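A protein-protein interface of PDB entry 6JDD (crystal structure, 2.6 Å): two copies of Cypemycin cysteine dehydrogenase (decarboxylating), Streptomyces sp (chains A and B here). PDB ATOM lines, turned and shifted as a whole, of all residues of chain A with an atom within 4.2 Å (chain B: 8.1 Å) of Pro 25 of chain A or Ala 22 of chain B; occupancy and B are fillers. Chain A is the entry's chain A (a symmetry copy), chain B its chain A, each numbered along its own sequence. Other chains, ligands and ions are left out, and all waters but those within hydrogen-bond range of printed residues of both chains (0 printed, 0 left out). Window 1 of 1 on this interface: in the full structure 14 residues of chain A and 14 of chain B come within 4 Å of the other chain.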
ATOM      1  N   ALA A  21      30.815 -11.516  -5.259  1.00  0.00           N
ATOM      2  CA  ALA A  21      31.368 -10.318  -5.928  1.00  0.00           C
ATOM      3  C   ALA A  21      31.063 -10.411  -7.417  1.00  0.00           C
ATOM      4  O   ALA A  21      30.860  -9.390  -7.990  1.00  0.00           O
ATOM      5  CB  ALA A  21      32.837 -10.167  -5.677  1.00  0.00           C
ATOM      6  N   ALA A  22      30.987 -11.619  -7.974  1.00  0.00           N
ATOM      7  CA  ALA A  22      30.654 -11.846  -9.401  1.00  0.00           C
ATOM      8  C   ALA A  22      29.284 -11.219  -9.747  1.00  0.00           C
ATOM      9  O   ALA A  22      29.117 -10.816 -10.929  1.00  0.00           O
ATOM     10  CB  ALA A  22      30.678 -13.308  -9.740  1.00  0.00           C
ATOM     11  N   LEU A  23      28.379 -11.127  -8.768  1.00  0.00           N
ATOM     12  CA  LEU A  23      26.995 -10.614  -8.922  1.00  0.00           C
ATOM     13  C   LEU A  23      26.915  -9.096  -8.707  1.00  0.00           C
ATOM     14  O   LEU A  23      25.879  -8.538  -9.003  1.00  0.00           O
ATOM     15  CB  LEU A  23      26.102 -11.303  -7.902  1.00  0.00           C
ATOM     16  CG  LEU A  23      25.471 -12.611  -8.348  1.00  0.00           C
ATOM     17  CD1 LEU A  23      26.485 -13.533  -8.972  1.00  0.00           C
ATOM     18  CD2 LEU A  23      24.820 -13.305  -7.158  1.00  0.00           C
ATOM     19  N   VAL A  24      27.969  -8.447  -8.217  1.00  0.00           N
ATOM     20  CA  VAL A  24      27.948  -7.008  -7.860  1.00  0.00           C
ATOM     21  C   VAL A  24      27.747  -6.165  -9.110  1.00  0.00           C
ATOM     22  O   VAL A  24      26.962  -5.238  -9.035  1.00  0.00           O
ATOM     23  CB  VAL A  24      29.204  -6.616  -7.071  1.00  0.00           C
ATOM     24  CG1 VAL A  24      29.336  -5.117  -6.866  1.00  0.00           C
ATOM     25  CG2 VAL A  24      29.171  -7.300  -5.737  1.00  0.00           C
ATOM     26  N   PRO A  25      28.428  -6.387 -10.270  1.00  0.00           N
ATOM     27  CA  PRO A  25      28.188  -5.543 -11.450  1.00  0.00           C
ATOM     28  C   PRO A  25      26.708  -5.471 -11.869  1.00  0.00           C
ATOM     29  O   PRO A  25      26.246  -4.401 -12.214  1.00  0.00           O
ATOM     30  CB  PRO A  25      29.005  -6.214 -12.542  1.00  0.00           C
ATOM     31  CG  PRO A  25      30.121  -6.887 -11.773  1.00  0.00           C
ATOM     32  CD  PRO A  25      29.461  -7.399 -10.523  1.00  0.00           C
ATOM     33  N   TRP A  26      25.984  -6.583 -11.756  1.00  0.00           N
ATOM     34  CA  TRP A  26      24.509  -6.589 -11.966  1.00  0.00           C
ATOM     35  C   TRP A  26      23.815  -5.618 -10.986  1.00  0.00           C
ATOM     36  O   TRP A  26      23.011  -4.774 -11.444  1.00  0.00           O
ATOM     37  CB  TRP A  26      23.961  -8.016 -11.859  1.00  0.00           C
ATOM     38  CG  TRP A  26      22.534  -8.133 -12.270  1.00  0.00           C
ATOM     39  CD1 TRP A  26      22.069  -8.520 -13.487  1.00  0.00           C
ATOM     40  CD2 TRP A  26      21.381  -7.844 -11.465  1.00  0.00           C
ATOM     41  NE1 TRP A  26      20.702  -8.508 -13.489  1.00  0.00           N
ATOM     42  CE2 TRP A  26      20.251  -8.094 -12.269  1.00  0.00           C
ATOM     43  CE3 TRP A  26      21.197  -7.413 -10.153  1.00  0.00           C
ATOM     44  CZ2 TRP A  26      18.952  -7.923 -11.815  1.00  0.00           C
ATOM     45  CZ3 TRP A  26      19.906  -7.256  -9.688  1.00  0.00           C
ATOM     46  CH2 TRP A  26      18.805  -7.516 -10.509  1.00  0.00           C
ATOM     47  N   TRP A  27      24.118  -5.713  -9.693  1.00  0.00           N
ATOM     48  CA  TRP A  27      23.553  -4.807  -8.657  1.00  0.00           C
ATOM     49  C   TRP A  27      23.992  -3.351  -8.848  1.00  0.00           C
ATOM     50  O   TRP A  27      23.181  -2.463  -8.623  1.00  0.00           O
ATOM     51  CB  TRP A  27      23.940  -5.306  -7.276  1.00  0.00           C
ATOM     52  CG  TRP A  27      23.109  -6.472  -6.899  1.00  0.00           C
ATOM     53  CD1 TRP A  27      23.467  -7.787  -6.893  1.00  0.00           C
ATOM     54  CD2 TRP A  27      21.722  -6.416  -6.570  1.00  0.00           C
ATOM     55  NE1 TRP A  27      22.400  -8.564  -6.534  1.00  0.00           N
ATOM     56  CE2 TRP A  27      21.312  -7.743  -6.323  1.00  0.00           C
ATOM     57  CE3 TRP A  27      20.805  -5.377  -6.448  1.00  0.00           C
ATOM     58  CZ2 TRP A  27      20.007  -8.054  -5.936  1.00  0.00           C
ATOM     59  CZ3 TRP A  27      19.508  -5.691  -6.086  1.00  0.00           C
ATOM     60  CH2 TRP A  27      19.120  -7.012  -5.823  1.00  0.00           C
ATOM     61  N   ILE A  28      25.244  -3.089  -9.193  1.00  0.00           N
ATOM     62  CA  ILE A  28      25.688  -1.701  -9.526  1.00  0.00           C
ATOM     63  C   ILE A  28      24.856  -1.199 -10.719  1.00  0.00           C
ATOM     64  O   ILE A  28      24.346  -0.068 -10.648  1.00  0.00           O
ATOM     65  CB  ILE A  28      27.198  -1.615  -9.821  1.00  0.00           C
ATOM     66  CG1 ILE A  28      28.057  -2.082  -8.639  1.00  0.00           C
ATOM     67  CG2 ILE A  28      27.572  -0.198 -10.274  1.00  0.00           C
ATOM     68  CD1 ILE A  28      27.944  -1.215  -7.425  1.00  0.00           C
ATOM     69  N   HIS A  29      24.700  -2.001 -11.775  1.00  0.00           N
ATOM     70  CA  HIS A  29      23.876  -1.631 -12.949  1.00  0.00           C
ATOM     71  C   HIS A  29      22.455  -1.305 -12.479  1.00  0.00           C
ATOM     72  O   HIS A  29      21.955  -0.249 -12.858  1.00  0.00           O
ATOM     73  CB  HIS A  29      23.917  -2.746 -13.984  1.00  0.00           C
ATOM     74  CG  HIS A  29      23.047  -2.469 -15.164  1.00  0.00           C
ATOM     75  ND1 HIS A  29      23.331  -1.430 -16.045  1.00  0.00           N
ATOM     76  CD2 HIS A  29      21.918  -3.068 -15.599  1.00  0.00           C
ATOM     77  CE1 HIS A  29      22.421  -1.416 -16.971  1.00  0.00           C
ATOM     78  NE2 HIS A  29      21.547  -2.408 -16.723  1.00  0.00           N
ATOM     79  N   ALA A  56      34.861  -3.604 -15.992  1.00  0.00           N
ATOM     80  CA  ALA A  56      33.398  -3.554 -16.155  1.00  0.00           C
ATOM     81  C   ALA A  56      32.790  -2.518 -15.180  1.00  0.00           C
ATOM     82  O   ALA A  56      31.870  -1.772 -15.592  1.00  0.00           O
ATOM     83  CB  ALA A  56      32.825  -4.937 -15.983  1.00  0.00           C
ATOM     84  N   LEU A  60      30.231   0.586 -15.553  1.00  0.00           N
ATOM     85  CA  LEU A  60      28.877   0.590 -14.962  1.00  0.00           C
ATOM     86  C   LEU A  60      28.751   1.672 -13.884  1.00  0.00           C
ATOM     87  O   LEU A  60      27.648   2.140 -13.684  1.00  0.00           O
ATOM     88  CB  LEU A  60      28.600  -0.801 -14.401  1.00  0.00           C
ATOM     89  CG  LEU A  60      28.612  -1.909 -15.450  1.00  0.00           C
ATOM     90  CD1 LEU A  60      28.714  -3.295 -14.822  1.00  0.00           C
ATOM     91  CD2 LEU A  60      27.383  -1.810 -16.343  1.00  0.00           C
ATOM     92  N   VAL B  15      29.676 -16.638 -24.249  1.00  0.00           N
ATOM     93  CA  VAL B  15      29.698 -15.243 -23.727  1.00  0.00           C
ATOM     94  C   VAL B  15      30.717 -14.452 -24.532  1.00  0.00           C
ATOM     95  O   VAL B  15      31.876 -14.901 -24.611  1.00  0.00           O
ATOM     96  CB  VAL B  15      30.046 -15.223 -22.231  1.00  0.00           C
ATOM     97  CG1 VAL B  15      29.915 -13.815 -21.633  1.00  0.00           C
ATOM     98  CG2 VAL B  15      29.220 -16.246 -21.459  1.00  0.00           C
ATOM     99  N   THR B  16      30.333 -13.286 -25.056  1.00  0.00           N
ATOM    100  CA  THR B  16      31.188 -12.460 -25.955  1.00  0.00           C
ATOM    101  C   THR B  16      31.322 -11.062 -25.353  1.00  0.00           C
ATOM    102  O   THR B  16      30.597 -10.752 -24.470  1.00  0.00           O
ATOM    103  CB  THR B  16      30.659 -12.444 -27.407  1.00  0.00           C
ATOM    104  OG1 THR B  16      29.511 -11.593 -27.516  1.00  0.00           O
ATOM    105  CG2 THR B  16      30.349 -13.826 -27.966  1.00  0.00           C
ATOM    106  N   GLY B  17      32.232 -10.255 -25.901  1.00  0.00           N
ATOM    107  CA  GLY B  17      32.854  -9.066 -25.289  1.00  0.00           C
ATOM    108  C   GLY B  17      32.008  -7.824 -25.381  1.00  0.00           C
ATOM    109  O   GLY B  17      32.454  -6.789 -25.913  1.00  0.00           O
ATOM    110  N   SER B  18      30.853  -7.853 -24.780  1.00  0.00           N
ATOM    111  CA  SER B  18      30.149  -6.592 -24.506  1.00  0.00           C
ATOM    112  C   SER B  18      30.081  -6.411 -22.994  1.00  0.00           C
ATOM    113  O   SER B  18      30.211  -7.400 -22.221  1.00  0.00           O
ATOM    114  CB  SER B  18      28.811  -6.569 -25.188  1.00  0.00           C
ATOM    115  OG  SER B  18      27.958  -7.563 -24.688  1.00  0.00           O
ATOM    116  N   ILE B  19      29.887  -5.176 -22.574  1.00  0.00           N
ATOM    117  CA  ILE B  19      29.809  -4.831 -21.132  1.00  0.00           C
ATOM    118  C   ILE B  19      28.693  -5.675 -20.481  1.00  0.00           C
ATOM    119  O   ILE B  19      28.872  -6.079 -19.322  1.00  0.00           O
ATOM    120  CB  ILE B  19      29.679  -3.306 -20.964  1.00  0.00           C
ATOM    121  CG1 ILE B  19      29.878  -2.914 -19.506  1.00  0.00           C
ATOM    122  CG2 ILE B  19      28.378  -2.790 -21.540  1.00  0.00           C
ATOM    123  CD1 ILE B  19      31.300  -3.213 -19.061  1.00  0.00           C
ATOM    124  N   SER B  20      27.654  -6.079 -21.211  1.00  0.00           N
ATOM    125  CA  SER B  20      26.621  -7.023 -20.703  1.00  0.00           C
ATOM    126  C   SER B  20      27.257  -8.331 -20.215  1.00  0.00           C
ATOM    127  O   SER B  20      26.610  -9.048 -19.470  1.00  0.00           O
ATOM    128  CB  SER B  20      25.566  -7.320 -21.721  1.00  0.00           C
ATOM    129  OG  SER B  20      24.940  -6.136 -22.168  1.00  0.00           O
ATOM    130  N   ALA B  21      28.453  -8.699 -20.657  1.00  0.00           N
ATOM    131  CA  ALA B  21      29.056  -9.962 -20.177  1.00  0.00           C
ATOM    132  C   ALA B  21      29.252  -9.863 -18.670  1.00  0.00           C
ATOM    133  O   ALA B  21      29.131 -10.865 -18.044  1.00  0.00           O
ATOM    134  CB  ALA B  21      30.343 -10.268 -20.880  1.00  0.00           C
ATOM    135  N   ALA B  22      29.489  -8.664 -18.140  1.00  0.00           N
ATOM    136  CA  ALA B  22      29.654  -8.427 -16.685  1.00  0.00           C
ATOM    137  C   ALA B  22      28.405  -8.907 -15.911  1.00  0.00           C
ATOM    138  O   ALA B  22      28.580  -9.310 -14.730  1.00  0.00           O
ATOM    139  CB  ALA B  22      29.945  -6.983 -16.398  1.00  0.00           C
ATOM    140  N   LEU B  23      27.232  -8.881 -16.550  1.00  0.00           N
ATOM    141  CA  LEU B  23      25.921  -9.241 -15.955  1.00  0.00           C
ATOM    142  C   LEU B  23      25.611 -10.738 -16.105  1.00  0.00           C
ATOM    143  O   LEU B  23      24.669 -11.184 -15.485  1.00  0.00           O
ATOM    144  CB  LEU B  23      24.832  -8.441 -16.650  1.00  0.00           C
ATOM    145  CG  LEU B  23      24.523  -7.080 -16.050  1.00  0.00           C
ATOM    146  CD1 LEU B  23      25.777  -6.286 -15.797  1.00  0.00           C
ATOM    147  CD2 LEU B  23      23.607  -6.297 -16.983  1.00  0.00           C
ATOM    148  N   VAL B  24      26.377 -11.490 -16.893  1.00  0.00           N
ATOM    149  CA  VAL B  24      26.086 -12.911 -17.200  1.00  0.00           C
ATOM    150  C   VAL B  24      26.202 -13.749 -15.936  1.00  0.00           C
ATOM    151  O   VAL B  24      25.337 -14.583 -15.741  1.00  0.00           O
ATOM    152  CB  VAL B  24      26.975 -13.424 -18.340  1.00  0.00           C
ATOM    153  CG1 VAL B  24      26.870 -14.925 -18.549  1.00  0.00           C
ATOM    154  CG2 VAL B  24      26.595 -12.716 -19.606  1.00  0.00           C
ATOM    155  N   PRO B  25      27.236 -13.624 -15.056  1.00  0.00           N
ATOM    156  CA  PRO B  25      27.292 -14.458 -13.846  1.00  0.00           C
ATOM    157  C   PRO B  25      26.024 -14.374 -12.978  1.00  0.00           C
ATOM    158  O   PRO B  25      25.581 -15.393 -12.484  1.00  0.00           O
ATOM    159  CB  PRO B  25      28.483 -13.900 -13.082  1.00  0.00           C
ATOM    160  CG  PRO B  25      29.363 -13.340 -14.178  1.00  0.00           C
ATOM    161  CD  PRO B  25      28.400 -12.736 -15.162  1.00  0.00           C
ATOM    162  N   TRP B  26      25.428 -13.188 -12.875  1.00  0.00           N
ATOM    163  CA  TRP B  26      24.107 -13.024 -12.206  1.00  0.00           C
ATOM    164  C   TRP B  26      23.035 -13.896 -12.897  1.00  0.00           C
ATOM    165  O   TRP B  26      22.330 -14.655 -12.192  1.00  0.00           O
ATOM    166  CB  TRP B  26      23.713 -11.544 -12.159  1.00  0.00           C
ATOM    167  CG  TRP B  26      22.512 -11.279 -11.318  1.00  0.00           C
ATOM    168  CD1 TRP B  26      22.504 -10.865 -10.024  1.00  0.00           C
ATOM    169  CD2 TRP B  26      21.139 -11.425 -11.709  1.00  0.00           C
ATOM    170  NE1 TRP B  26      21.216 -10.727  -9.588  1.00  0.00           N
ATOM    171  CE2 TRP B  26      20.358 -11.067 -10.593  1.00  0.00           C
ATOM    172  CE3 TRP B  26      20.501 -11.809 -12.887  1.00  0.00           C
ATOM    173  CZ2 TRP B  26      18.971 -11.086 -10.607  1.00  0.00           C
ATOM    174  CZ3 TRP B  26      19.121 -11.816 -12.915  1.00  0.00           C
ATOM    175  CH2 TRP B  26      18.373 -11.451 -11.791  1.00  0.00           C
ATOM    176  N   TRP B  27      22.920 -13.811 -14.221  1.00  0.00           N
ATOM    177  CA  TRP B  27      21.959 -14.631 -15.008  1.00  0.00           C
ATOM    178  C   TRP B  27      22.273 -16.129 -14.940  1.00  0.00           C
ATOM    179  O   TRP B  27      21.341 -16.919 -14.879  1.00  0.00           O
ATOM    180  CB  TRP B  27      21.939 -14.153 -16.449  1.00  0.00           C
ATOM    181  CG  TRP B  27      21.164 -12.895 -16.563  1.00  0.00           C
ATOM    182  CD1 TRP B  27      21.644 -11.629 -16.705  1.00  0.00           C
ATOM    183  CD2 TRP B  27      19.747 -12.794 -16.433  1.00  0.00           C
ATOM    184  NE1 TRP B  27      20.610 -10.732 -16.721  1.00  0.00           N
ATOM    185  CE2 TRP B  27      19.428 -11.425 -16.560  1.00  0.00           C
ATOM    186  CE3 TRP B  27      18.731 -13.723 -16.239  1.00  0.00           C
ATOM    187  CZ2 TRP B  27      18.110 -10.966 -16.518  1.00  0.00           C
ATOM    188  CZ3 TRP B  27      17.430 -13.263 -16.175  1.00  0.00           C
ATOM    189  CH2 TRP B  27      17.125 -11.903 -16.324  1.00  0.00           C
ATOM    190  N   ALA B  48      35.440 -11.070 -23.714  1.00  0.00           N
ATOM    191  CA  ALA B  48      34.435 -11.126 -22.619  1.00  0.00           C
ATOM    192  C   ALA B  48      35.152 -11.303 -21.277  1.00  0.00           C
ATOM    193  O   ALA B  48      34.632 -10.886 -20.241  1.00  0.00           O
ATOM    194  CB  ALA B  48      33.479 -12.263 -22.858  1.00  0.00           C
ATOM    195  N   ARG B  50      37.618  -9.823 -20.270  1.00  0.00           N
ATOM    196  CA  ARG B  50      38.016  -8.491 -19.740  1.00  0.00           C
ATOM    197  C   ARG B  50      36.844  -7.889 -18.973  1.00  0.00           C
ATOM    198  O   ARG B  50      37.062  -6.855 -18.363  1.00  0.00           O
ATOM    199  CB  ARG B  50      38.411  -7.504 -20.857  1.00  0.00           C
ATOM    200  CG  ARG B  50      39.675  -7.869 -21.641  1.00  0.00           C
ATOM    201  CD  ARG B  50      40.004  -6.884 -22.785  1.00  0.00           C
ATOM    202  NE  ARG B  50      39.057  -6.809 -23.926  1.00  0.00           N
ATOM    203  CZ  ARG B  50      39.363  -6.912 -25.251  1.00  0.00           C
ATOM    204  NH1 ARG B  50      40.606  -7.105 -25.656  1.00  0.00           N
ATOM    205  NH2 ARG B  50      38.414  -6.830 -26.185  1.00  0.00           N
ATOM    206  N   PHE B  51      35.635  -8.453 -19.099  1.00  0.00           N
ATOM    207  CA  PHE B  51      34.413  -7.875 -18.475  1.00  0.00           C
ATOM    208  C   PHE B  51      33.838  -8.792 -17.400  1.00  0.00           C
ATOM    209  O   PHE B  51      32.992  -8.329 -16.616  1.00  0.00           O
ATOM    210  CB  PHE B  51      33.368  -7.534 -19.530  1.00  0.00           C
ATOM    211  CG  PHE B  51      33.805  -6.443 -20.479  1.00  0.00           C
ATOM    212  CD1 PHE B  51      34.401  -5.275 -20.012  1.00  0.00           C
ATOM    213  CD2 PHE B  51      33.625  -6.585 -21.853  1.00  0.00           C
ATOM    214  CE1 PHE B  51      34.794  -4.283 -20.896  1.00  0.00           C
ATOM    215  CE2 PHE B  51      34.041  -5.610 -22.740  1.00  0.00           C
ATOM    216  CZ  PHE B  51      34.624  -4.462 -22.258  1.00  0.00           C
ATOM    217  N   LEU B  52      34.291 -10.038 -17.356  1.00  0.00           N
ATOM    218  CA  LEU B  52      33.918 -10.952 -16.256  1.00  0.00           C
ATOM    219  C   LEU B  52      35.104 -11.843 -15.901  1.00  0.00           C
ATOM    220  O   LEU B  52      36.118 -11.772 -16.584  1.00  0.00           O
ATOM    221  CB  LEU B  52      32.677 -11.747 -16.640  1.00  0.00           C
ATOM    222  CG  LEU B  52      32.792 -12.654 -17.848  1.00  0.00           C
ATOM    223  CD1 LEU B  52      33.731 -13.805 -17.580  1.00  0.00           C
ATOM    224  CD2 LEU B  52      31.422 -13.208 -18.181  1.00  0.00           C
ATOM    225  N   ALA B  53      34.974 -12.627 -14.834  1.00  0.00           N
ATOM    226  CA  ALA B  53      36.020 -13.559 -14.396  1.00  0.00           C
ATOM    227  C   ALA B  53      35.561 -14.982 -14.728  1.00  0.00           C
ATOM    228  O   ALA B  53      34.512 -15.427 -14.213  1.00  0.00           O
ATOM    229  CB  ALA B  53      36.287 -13.327 -12.932  1.00  0.00           C
ATOM    230  N   PHE B  93      25.242 -15.147 -25.551  1.00  0.00           N
ATOM    231  CA  PHE B  93      24.627 -14.338 -24.475  1.00  0.00           C
ATOM    232  C   PHE B  93      25.726 -13.650 -23.689  1.00  0.00           C
ATOM    233  O   PHE B  93      26.420 -14.315 -22.930  1.00  0.00           O
ATOM    234  CB  PHE B  93      23.803 -15.242 -23.556  1.00  0.00           C
ATOM    235  CG  PHE B  93      23.039 -14.503 -22.491  1.00  0.00           C
ATOM    236  CD1 PHE B  93      21.995 -13.661 -22.829  1.00  0.00           C
ATOM    237  CD2 PHE B  93      23.373 -14.645 -21.162  1.00  0.00           C
ATOM    238  CE1 PHE B  93      21.298 -12.965 -21.859  1.00  0.00           C
ATOM    239  CE2 PHE B  93      22.669 -13.950 -20.194  1.00  0.00           C
ATOM    240  CZ  PHE B  93      21.633 -13.109 -20.538  1.00  0.00           C
ATOM    241  N   PRO B  94      26.030 -12.362 -23.930  1.00  0.00           N
ATOM    242  CA  PRO B  94      25.562 -11.634 -25.104  1.00  0.00           C
ATOM    243  C   PRO B  94      26.342 -11.922 -26.393  1.00  0.00           C
ATOM    244  O   PRO B  94      27.368 -12.581 -26.340  1.00  0.00           O
ATOM    245  CB  PRO B  94      25.859 -10.198 -24.702  1.00  0.00           C
ATOM    246  CG  PRO B  94      27.155 -10.316 -23.965  1.00  0.00           C
ATOM    247  CD  PRO B  94      26.976 -11.575 -23.144  1.00  0.00           C
ATOM    248  N   PHE B 170      19.398  -8.921 -25.380  1.00  0.00           N
ATOM    249  CA  PHE B 170      19.984  -9.453 -24.112  1.00  0.00           C
ATOM    250  C   PHE B 170      18.887 -10.004 -23.195  1.00  0.00           C
ATOM    251  O   PHE B 170      18.538  -9.383 -22.191  1.00  0.00           O
ATOM    252  CB  PHE B 170      20.817  -8.404 -23.367  1.00  0.00           C
ATOM    253  CG  PHE B 170      21.702  -9.021 -22.322  1.00  0.00           C
ATOM    254  CD1 PHE B 170      22.620 -10.004 -22.676  1.00  0.00           C
ATOM    255  CD2 PHE B 170      21.602  -8.639 -20.991  1.00  0.00           C
ATOM    256  CE1 PHE B 170      23.439 -10.576 -21.722  1.00  0.00           C
ATOM    257  CE2 PHE B 170      22.425  -9.206 -20.038  1.00  0.00           C
ATOM    258  CZ  PHE B 170      23.328 -10.183 -20.408  1.00  0.00           C
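Of the 11 printed residues of chain A, 7 touch a printed residue of chain B. Printed residues of chain B that touch a printed residue of chain A: Ile 19, Ala 22, Leu 23, Pro 25, Trp 26, Trp 27 and Phe 51. Among the printed residues, 11 pairs touch across the chains. Among the printed residues, no Asp or Glu carboxylate lies within 4 Å of a Lys or Arg side-chain nitrogen of the other chain.
Of the printed residues of chain B, Pro 25 of chain A touches Ala 22. Printed residues of chain B within 4 Å of His 29 of chain A: Leu 23. Of the printed residues of chain A, Ile 19 of chain B touches Ala 56 (3.6 Å). Of chain A, only Pro 25 (3.8 Å) and Ala 56 (3.6 Å) come within 4 Å of Ala 22 of chain B. Printed residues of chain A within 4 Å of Leu 23 of chain B: Trp 26 and His 29. Printed residues of chain A within 4 Å of Trp 27 of chain B: Trp 26. Printed residues of chain A within 4 Å of Phe 51 of chain B: Ala 56. The nearest residue of chain B that does not touch Pro 25 of chain A is Leu 23 of chain B (4.1 Å). The nearest printed residue of chain B that does not touch Trp 26 of chain A is Ala 22 of chain B (4.8 Å).
Ala 22 of chain A touches Pro 25 of chain B (O to CB, 3.8 Å). CG of Leu 23 of chain A touches CD1 of Trp 26 of chain B, at 3.8 Å. Ala 22 of chain B touches Pro 25 of chain A. CG of Leu 23 of chain B touches CD1 of Trp 26 of chain A, 3.8 Å away. Trp 26 of chain B touches Trp 26 of chain A. NE1 of Trp 26 of chain A touches NE1 of Trp 27 of chain B (3.9 Å). NE1 of Trp 27 of chain A touches NE1 of Trp 26 of chain B, at 3.9 Å. Ile 19 of chain B touches Ala 56 of chain A (CD1 to CA, 3.6 Å). CB of Ala 56 of chain A touches CB of Ala 22 of chain B, at 3.6 Å. Phe 51 of chain B touches Ala 56 of chain A (O to CB, 3.5 Å).
Ala 22 of chain A touches Pro 25 of chain B, and with the chains exchanged Pro 25 of chain A touches Ala 22 of chain B. Leu 23 of chain A touches Trp 26 of chain B, and with the chains exchanged Trp 26 of chain A touches Leu 23 of chain B. Trp 26 of chain B touches its own counterpart, Trp 26 of chain A. Trp 26 of chain A touches Trp 27 of chain B, and with the chains exchanged Trp 27 of chain A touches Trp 26 of chain B. Of the 11 pairs that touch across the chains among the printed residues, 7 have their exchanged pair printed and touching as well.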
